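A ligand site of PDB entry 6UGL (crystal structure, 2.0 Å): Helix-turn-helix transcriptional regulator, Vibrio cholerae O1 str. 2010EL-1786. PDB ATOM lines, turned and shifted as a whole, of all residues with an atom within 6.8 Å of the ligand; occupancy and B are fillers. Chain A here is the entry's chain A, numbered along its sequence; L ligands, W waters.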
ATOM      1  N   LYS A  23      20.652  -4.043  -9.064  1.00  0.00           N
ATOM      2  CA  LYS A  23      21.155  -5.344  -8.646  1.00  0.00           C
ATOM      3  C   LYS A  23      22.146  -5.120  -7.510  1.00  0.00           C
ATOM      4  O   LYS A  23      22.655  -4.011  -7.331  1.00  0.00           O
ATOM      5  CB  LYS A  23      21.869  -6.087  -9.804  1.00  0.00           C
ATOM      6  CG  LYS A  23      21.203  -5.990 -11.159  1.00  0.00           C
ATOM      7  CD  LYS A  23      22.223  -6.359 -12.257  1.00  0.00           C
ATOM      8  CE  LYS A  23      21.749  -6.031 -13.671  1.00  0.00           C
ATOM      9  NZ  LYS A  23      22.751  -6.465 -14.729  1.00  0.00           N
ATOM     10  N   PHE A  29      19.384  -9.449  -9.057  1.00  0.00           N
ATOM     11  CA  PHE A  29      18.361  -8.406  -9.170  1.00  0.00           C
ATOM     12  C   PHE A  29      17.709  -8.112  -7.817  1.00  0.00           C
ATOM     13  O   PHE A  29      17.299  -9.015  -7.092  1.00  0.00           O
ATOM     14  CB  PHE A  29      17.298  -8.817 -10.187  1.00  0.00           C
ATOM     15  CG  PHE A  29      17.646  -8.467 -11.618  1.00  0.00           C
ATOM     16  CD1 PHE A  29      18.770  -8.998 -12.232  1.00  0.00           C
ATOM     17  CD2 PHE A  29      16.841  -7.603 -12.349  1.00  0.00           C
ATOM     18  CE1 PHE A  29      19.082  -8.676 -13.540  1.00  0.00           C
ATOM     19  CE2 PHE A  29      17.154  -7.268 -13.664  1.00  0.00           C
ATOM     20  CZ  PHE A  29      18.274  -7.795 -14.257  1.00  0.00           C
ATOM     21  N   TYR A  36      10.909  -3.215 -17.723  1.00  0.00           N
ATOM     22  CA  TYR A  36      12.041  -4.111 -17.904  1.00  0.00           C
ATOM     23  C   TYR A  36      11.612  -5.579 -17.793  1.00  0.00           C
ATOM     24  O   TYR A  36      12.009  -6.417 -18.608  1.00  0.00           O
ATOM     25  CB  TYR A  36      13.173  -3.791 -16.911  1.00  0.00           C
ATOM     26  CG  TYR A  36      14.338  -4.733 -17.142  1.00  0.00           C
ATOM     27  CD1 TYR A  36      15.343  -4.424 -18.056  1.00  0.00           C
ATOM     28  CD2 TYR A  36      14.420  -5.962 -16.480  1.00  0.00           C
ATOM     29  CE1 TYR A  36      16.385  -5.270 -18.294  1.00  0.00           C
ATOM     30  CE2 TYR A  36      15.471  -6.830 -16.712  1.00  0.00           C
ATOM     31  CZ  TYR A  36      16.453  -6.484 -17.619  1.00  0.00           C
ATOM     32  OH  TYR A  36      17.499  -7.324 -17.875  1.00  0.00           O
ATOM     33  N   LEU A  39       9.878  -6.634 -20.968  1.00  0.00           N
ATOM     34  CA  LEU A  39      10.891  -6.766 -22.016  1.00  0.00           C
ATOM     35  C   LEU A  39      11.587  -8.121 -21.969  1.00  0.00           C
ATOM     36  O   LEU A  39      11.781  -8.766 -23.002  1.00  0.00           O
ATOM     37  CB  LEU A  39      11.929  -5.666 -21.870  1.00  0.00           C
ATOM     38  CG  LEU A  39      13.110  -5.689 -22.849  1.00  0.00           C
ATOM     39  CD1 LEU A  39      12.626  -5.476 -24.302  1.00  0.00           C
ATOM     40  CD2 LEU A  39      14.170  -4.634 -22.467  1.00  0.00           C
ATOM     41  N   ILE A  40      11.932  -8.559 -20.754  1.00  0.00           N
ATOM     42  CA  ILE A  40      12.849  -9.649 -20.474  1.00  0.00           C
ATOM     43  C   ILE A  40      12.053 -10.945 -20.343  1.00  0.00           C
ATOM     44  O   ILE A  40      12.586 -12.004 -19.993  1.00  0.00           O
ATOM     45  CB  ILE A  40      13.687  -9.306 -19.215  1.00  0.00           C
ATOM     46  CG1 ILE A  40      15.138  -9.735 -19.400  1.00  0.00           C
ATOM     47  CG2 ILE A  40      13.084  -9.881 -17.948  1.00  0.00           C
ATOM     48  CD1 ILE A  40      15.818  -8.999 -20.516  1.00  0.00           C
ATOM     49  N   ASP A  53      21.268 -12.296 -14.289  1.00  0.00           N
ATOM     50  CA  ASP A  53      21.048 -12.139 -15.725  1.00  0.00           C
ATOM     51  C   ASP A  53      21.079 -13.494 -16.444  1.00  0.00           C
ATOM     52  O   ASP A  53      20.423 -13.647 -17.479  1.00  0.00           O
ATOM     53  CB  ASP A  53      22.102 -11.201 -16.307  1.00  0.00           C
ATOM     54  CG  ASP A  53      21.943  -9.770 -15.815  1.00  0.00           C
ATOM     55  OD1 ASP A  53      20.936  -9.128 -16.198  1.00  0.00           O
ATOM     56  OD2 ASP A  53      22.824  -9.310 -15.055  1.00  0.00           O
ATOM     57  N   THR A  60      18.912 -12.416 -23.968  1.00  0.00           N
ATOM     58  CA  THR A  60      19.882 -11.525 -23.335  1.00  0.00           C
ATOM     59  C   THR A  60      20.796 -12.263 -22.361  1.00  0.00           C
ATOM     60  O   THR A  60      21.964 -11.874 -22.172  1.00  0.00           O
ATOM     61  CB  THR A  60      19.162 -10.397 -22.572  1.00  0.00           C
ATOM     62  OG1 THR A  60      18.152 -10.963 -21.706  1.00  0.00           O
ATOM     63  CG2 THR A  60      18.526  -9.430 -23.535  1.00  0.00           C
ATOM     64  N   CYS A  63      24.415 -12.961 -23.004  1.00  0.00           N
ATOM     65  CA  CYS A  63      25.416 -11.945 -22.720  1.00  0.00           C
ATOM     66  C   CYS A  63      25.531 -11.646 -21.230  1.00  0.00           C
ATOM     67  O   CYS A  63      26.089 -10.605 -20.838  1.00  0.00           O
ATOM     68  CB  CYS A  63      25.103 -10.669 -23.502  1.00  0.00           C
ATOM     69  SG  CYS A  63      25.173 -10.905 -25.298  1.00  0.00           S
ATOM     70  N   PHE A  67      27.282  -8.389 -19.090  1.00  0.00           N
ATOM     71  CA  PHE A  67      26.564  -7.574 -18.113  1.00  0.00           C
ATOM     72  C   PHE A  67      27.303  -7.552 -16.782  1.00  0.00           C
ATOM     73  O   PHE A  67      27.511  -6.495 -16.190  1.00  0.00           O
ATOM     74  CB  PHE A  67      25.137  -8.081 -17.933  1.00  0.00           C
ATOM     75  CG  PHE A  67      24.336  -8.155 -19.208  1.00  0.00           C
ATOM     76  CD1 PHE A  67      24.728  -7.466 -20.355  1.00  0.00           C
ATOM     77  CD2 PHE A  67      23.180  -8.947 -19.263  1.00  0.00           C
ATOM     78  CE1 PHE A  67      23.985  -7.557 -21.517  1.00  0.00           C
ATOM     79  CE2 PHE A  67      22.428  -9.027 -20.434  1.00  0.00           C
ATOM     80  CZ  PHE A  67      22.839  -8.349 -21.570  1.00  0.00           C
ATOM     81  N   GLN A  68      27.741  -8.729 -16.307  1.00  0.00           N
ATOM     82  CA  GLN A  68      28.395  -8.770 -15.002  1.00  0.00           C
ATOM     83  C   GLN A  68      29.744  -8.031 -15.030  1.00  0.00           C
ATOM     84  O   GLN A  68      30.104  -7.363 -14.058  1.00  0.00           O
ATOM     85  CB  GLN A  68      28.562 -10.220 -14.528  1.00  0.00           C
ATOM     86  CG  GLN A  68      27.228 -10.879 -14.194  1.00  0.00           C
ATOM     87  CD  GLN A  68      27.368 -12.283 -13.595  1.00  0.00           C
ATOM     88  OE1 GLN A  68      28.383 -12.950 -13.773  1.00  0.00           O
ATOM     89  NE2 GLN A  68      26.331 -12.729 -12.901  1.00  0.00           N
ATOM     90  N   GLN A  70      30.502  -5.471 -16.902  1.00  0.00           N
ATOM     91  CA  GLN A  70      30.098  -4.073 -16.833  1.00  0.00           C
ATOM     92  C   GLN A  70      29.772  -3.682 -15.394  1.00  0.00           C
ATOM     93  O   GLN A  70      30.342  -2.712 -14.861  1.00  0.00           O
ATOM     94  CB  GLN A  70      28.887  -3.857 -17.751  1.00  0.00           C
ATOM     95  CG  GLN A  70      29.201  -4.131 -19.200  1.00  0.00           C
ATOM     96  CD  GLN A  70      27.972  -4.350 -20.031  1.00  0.00           C
ATOM     97  OE1 GLN A  70      26.842  -4.288 -19.530  1.00  0.00           O
ATOM     98  NE2 GLN A  70      28.179  -4.620 -21.309  1.00  0.00           N
ATOM     99  N   ASP A  71      28.867  -4.422 -14.762  1.00  0.00           N
ATOM    100  CA  ASP A  71      28.485  -4.167 -13.377  1.00  0.00           C
ATOM    101  C   ASP A  71      29.698  -4.070 -12.457  1.00  0.00           C
ATOM    102  O   ASP A  71      29.826  -3.139 -11.665  1.00  0.00           O
ATOM    103  CB  ASP A  71      27.546  -5.267 -12.884  1.00  0.00           C
ATOM    104  CG  ASP A  71      26.233  -5.287 -13.630  1.00  0.00           C
ATOM    105  OD1 ASP A  71      26.031  -4.424 -14.504  1.00  0.00           O
ATOM    106  OD2 ASP A  71      25.404  -6.183 -13.340  1.00  0.00           O
ATOM    107  N   VAL A  83      26.092   1.596 -22.173  1.00  0.00           N
ATOM    108  CA  VAL A  83      26.240   0.329 -22.873  1.00  0.00           C
ATOM    109  C   VAL A  83      25.298   0.302 -24.067  1.00  0.00           C
ATOM    110  O   VAL A  83      24.102   0.561 -23.903  1.00  0.00           O
ATOM    111  CB  VAL A  83      25.978  -0.882 -21.945  1.00  0.00           C
ATOM    112  CG1 VAL A  83      26.276  -2.180 -22.677  1.00  0.00           C
ATOM    113  CG2 VAL A  83      26.817  -0.766 -20.660  1.00  0.00           C
ATOM    114  N   ASP A  85      23.294  -2.046 -26.171  1.00  0.00           N
ATOM    115  CA  ASP A  85      22.761  -3.379 -26.018  1.00  0.00           C
ATOM    116  C   ASP A  85      21.853  -3.698 -27.199  1.00  0.00           C
ATOM    117  O   ASP A  85      20.889  -2.963 -27.459  1.00  0.00           O
ATOM    118  CB  ASP A  85      22.012  -3.502 -24.696  1.00  0.00           C
ATOM    119  CG  ASP A  85      22.929  -3.947 -23.578  1.00  0.00           C
ATOM    120  OD1 ASP A  85      23.461  -5.069 -23.696  1.00  0.00           O
ATOM    121  OD2 ASP A  85      23.116  -3.165 -22.617  1.00  0.00           O
ATOM    122  N   HIS A  87      19.932  -7.096 -28.905  1.00  0.00           N
ATOM    123  CA  HIS A  87      19.612  -8.486 -28.598  1.00  0.00           C
ATOM    124  C   HIS A  87      18.278  -8.851 -29.208  1.00  0.00           C
ATOM    125  O   HIS A  87      17.392  -7.995 -29.320  1.00  0.00           O
ATOM    126  CB  HIS A  87      19.543  -8.763 -27.087  1.00  0.00           C
ATOM    127  CG  HIS A  87      20.691  -8.228 -26.292  1.00  0.00           C
ATOM    128  ND1 HIS A  87      21.751  -9.002 -25.907  1.00  0.00           N
ATOM    129  CD2 HIS A  87      20.928  -6.990 -25.810  1.00  0.00           C
ATOM    130  CE1 HIS A  87      22.612  -8.260 -25.225  1.00  0.00           C
ATOM    131  NE2 HIS A  87      22.126  -7.040 -25.142  1.00  0.00           N
ATOM    132  N   TYR A  89      14.810 -10.661 -28.335  1.00  0.00           N
ATOM    133  CA  TYR A  89      14.103 -10.722 -27.071  1.00  0.00           C
ATOM    134  C   TYR A  89      12.948 -11.717 -27.113  1.00  0.00           C
ATOM    135  O   TYR A  89      12.535 -12.158 -28.197  1.00  0.00           O
ATOM    136  CB  TYR A  89      13.587  -9.325 -26.673  1.00  0.00           C
ATOM    137  CG  TYR A  89      14.660  -8.467 -26.039  1.00  0.00           C
ATOM    138  CD1 TYR A  89      15.576  -7.757 -26.816  1.00  0.00           C
ATOM    139  CD2 TYR A  89      14.752  -8.337 -24.658  1.00  0.00           C
ATOM    140  CE1 TYR A  89      16.549  -6.975 -26.237  1.00  0.00           C
ATOM    141  CE2 TYR A  89      15.715  -7.546 -24.078  1.00  0.00           C
ATOM    142  CZ  TYR A  89      16.612  -6.868 -24.858  1.00  0.00           C
ATOM    143  OH  TYR A  89      17.580  -6.083 -24.258  1.00  0.00           O
ATOM    144  N   HIS A  97      19.164  -0.784 -27.229  1.00  0.00           N
ATOM    145  CA  HIS A  97      19.066   0.191 -26.150  1.00  0.00           C
ATOM    146  C   HIS A  97      20.441   0.742 -25.848  1.00  0.00           C
ATOM    147  O   HIS A  97      21.458   0.104 -26.090  1.00  0.00           O
ATOM    148  CB  HIS A  97      18.496  -0.402 -24.850  1.00  0.00           C
ATOM    149  CG  HIS A  97      17.136  -1.013 -24.977  1.00  0.00           C
ATOM    150  ND1 HIS A  97      16.935  -2.259 -25.529  1.00  0.00           N
ATOM    151  CD2 HIS A  97      15.926  -0.609 -24.526  1.00  0.00           C
ATOM    152  CE1 HIS A  97      15.658  -2.577 -25.453  1.00  0.00           C
ATOM    153  NE2 HIS A  97      15.017  -1.593 -24.855  1.00  0.00           N
ATOM    154  N   PHE A  99      21.897   1.377 -22.282  1.00  0.00           N
ATOM    155  CA  PHE A  99      21.700   1.166 -20.852  1.00  0.00           C
ATOM    156  C   PHE A  99      22.765   1.976 -20.129  1.00  0.00           C
ATOM    157  O   PHE A  99      23.960   1.787 -20.389  1.00  0.00           O
ATOM    158  CB  PHE A  99      21.798  -0.324 -20.480  1.00  0.00           C
ATOM    159  CG  PHE A  99      20.493  -1.076 -20.606  1.00  0.00           C
ATOM    160  CD1 PHE A  99      20.099  -1.636 -21.819  1.00  0.00           C
ATOM    161  CD2 PHE A  99      19.637  -1.208 -19.501  1.00  0.00           C
ATOM    162  CE1 PHE A  99      18.902  -2.320 -21.934  1.00  0.00           C
ATOM    163  CE2 PHE A  99      18.427  -1.886 -19.606  1.00  0.00           C
ATOM    164  CZ  PHE A  99      18.057  -2.449 -20.836  1.00  0.00           C
ATOM    165  N   LYS A 101      24.618   2.618 -16.650  1.00  0.00           N
ATOM    166  CA  LYS A 101      24.895   1.878 -15.424  1.00  0.00           C
ATOM    167  C   LYS A 101      25.686   2.767 -14.476  1.00  0.00           C
ATOM    168  O   LYS A 101      26.716   3.322 -14.861  1.00  0.00           O
ATOM    169  CB  LYS A 101      25.633   0.564 -15.719  1.00  0.00           C
ATOM    170  CG  LYS A 101      24.801  -0.452 -16.458  1.00  0.00           C
ATOM    171  CD  LYS A 101      25.561  -1.779 -16.667  1.00  0.00           C
ATOM    172  CE  LYS A 101      24.634  -2.893 -17.093  1.00  0.00           C
ATOM    173  NZ  LYS A 101      25.361  -4.209 -17.241  1.00  0.00           N
ATOM    174  N   PHE A 116      20.689   0.270 -13.265  1.00  0.00           N
ATOM    175  CA  PHE A 116      20.662   0.240 -14.719  1.00  0.00           C
ATOM    176  C   PHE A 116      19.451   1.001 -15.214  1.00  0.00           C
ATOM    177  O   PHE A 116      18.381   0.964 -14.603  1.00  0.00           O
ATOM    178  CB  PHE A 116      20.664  -1.191 -15.297  1.00  0.00           C
ATOM    179  CG  PHE A 116      19.513  -2.058 -14.840  1.00  0.00           C
ATOM    180  CD1 PHE A 116      19.634  -2.831 -13.688  1.00  0.00           C
ATOM    181  CD2 PHE A 116      18.318  -2.107 -15.560  1.00  0.00           C
ATOM    182  CE1 PHE A 116      18.586  -3.633 -13.244  1.00  0.00           C
ATOM    183  CE2 PHE A 116      17.260  -2.910 -15.118  1.00  0.00           C
ATOM    184  CZ  PHE A 116      17.400  -3.682 -13.962  1.00  0.00           C
ATOM    185  N   SER A 229      26.879  -6.517 -26.530  1.00  0.00           N
ATOM    186  CA  SER A 229      26.776  -5.638 -25.375  1.00  0.00           C
ATOM    187  C   SER A 229      28.160  -5.027 -25.169  1.00  0.00           C
ATOM    188  O   SER A 229      29.045  -5.662 -24.596  1.00  0.00           O
ATOM    189  CB  SER A 229      26.316  -6.402 -24.137  1.00  0.00           C
ATOM    190  OG  SER A 229      26.269  -5.577 -22.998  1.00  0.00           O
HETATM  191  C1  LIG L   1      21.280  -5.429 -20.567  1.00  0.00           C
HETATM  192  C2  LIG L   1      19.935  -5.767 -20.265  1.00  0.00           C
HETATM  193  C3  LIG L   1      20.450  -5.566 -17.997  1.00  0.00           C
HETATM  194  C4  LIG L   1      21.776  -5.393 -18.385  1.00  0.00           C
HETATM  195  C5  LIG L   1      18.936  -6.069 -21.352  1.00  0.00           C
HETATM  196  C6  LIG L   1      20.011  -5.538 -16.564  1.00  0.00           C
HETATM  197  N1  LIG L   1      22.214  -5.192 -19.598  1.00  0.00           N
HETATM  198  N2  LIG L   1      19.566  -5.843 -18.957  1.00  0.00           N
HETATM  199  O1  LIG L   1      22.656  -5.402 -17.375  1.00  0.00           O
HETATM  200  O   HOH W   1      24.498  -3.909 -20.621  1.00  0.00           O
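The side-chain amino group (NZ) of Lys 23 lies within hydrogen-bond range of an oxygen (O1) of the ligand.
The side-chain amino group (NZ) of Lys 101 is in hydrogen-bond range of an oxygen (O1) of the ligand.
OH of Tyr 36 lies within hydrogen-bond range of N2 of the ligand (2.8 Å).
OD1 of Asp 85 is in hydrogen-bond range of OG of Ser 229 (2.9 Å).
NZ of Lys 101 lies within hydrogen-bond range of O of Phe 67 (3.3 Å).
The side-chain amino group of Lys 101 is in hydrogen-bond range of the side-chain amide oxygen of Gln 70 (2.7 Å).
NZ of Lys 23 lies within salt-bridge range of OD2 of Asp 71 (3.0 Å).
The backbone carbonyl oxygen (O) of Phe 99 is in hydrogen-bond range of the backbone NH (N) of Val 83 (2.8 Å).
The backbone carbonyl oxygen of Asp 85 lies within hydrogen-bond range of the backbone NH of His 97 (2.8 Å).
The side-chain carboxylate of Asp 85 sits at hydrogen-bond distance from a ring nitrogen (NE2) of His 87.
The side-chain amino group (NZ) of Lys 101 lies within salt-bridge range of the side-chain carboxylate (OD1) of Asp 71 (2.8 Å).
Residues that only touch the ligand: Tyr 89 (3.2 Å), Phe 67 (3.5 Å), Asp 85 (3.6 Å), Phe 29 (3.7 Å), Asp 53 (3.7 Å), Phe 99 (3.8 Å) and Phe 116 (3.9 Å).
Hydrophobic or aromatic side chains that line the ligand: Phe 29, Tyr 36, Phe 67, Phe 99 and Phe 116.
Along chain A the residues within 4 Å of the ligand span positions 23 to 116.
The nearest printed residue that does not touch the ligand is Thr 60 (4.03 Å).
Water W1 lies within hydrogen-bond range of OD2 of Asp 85 (2.5 Å), OE1 of Gln 70 (2.6 Å), N1 of the ligand (2.8 Å) and OG of Ser 229 (3.4 Å).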
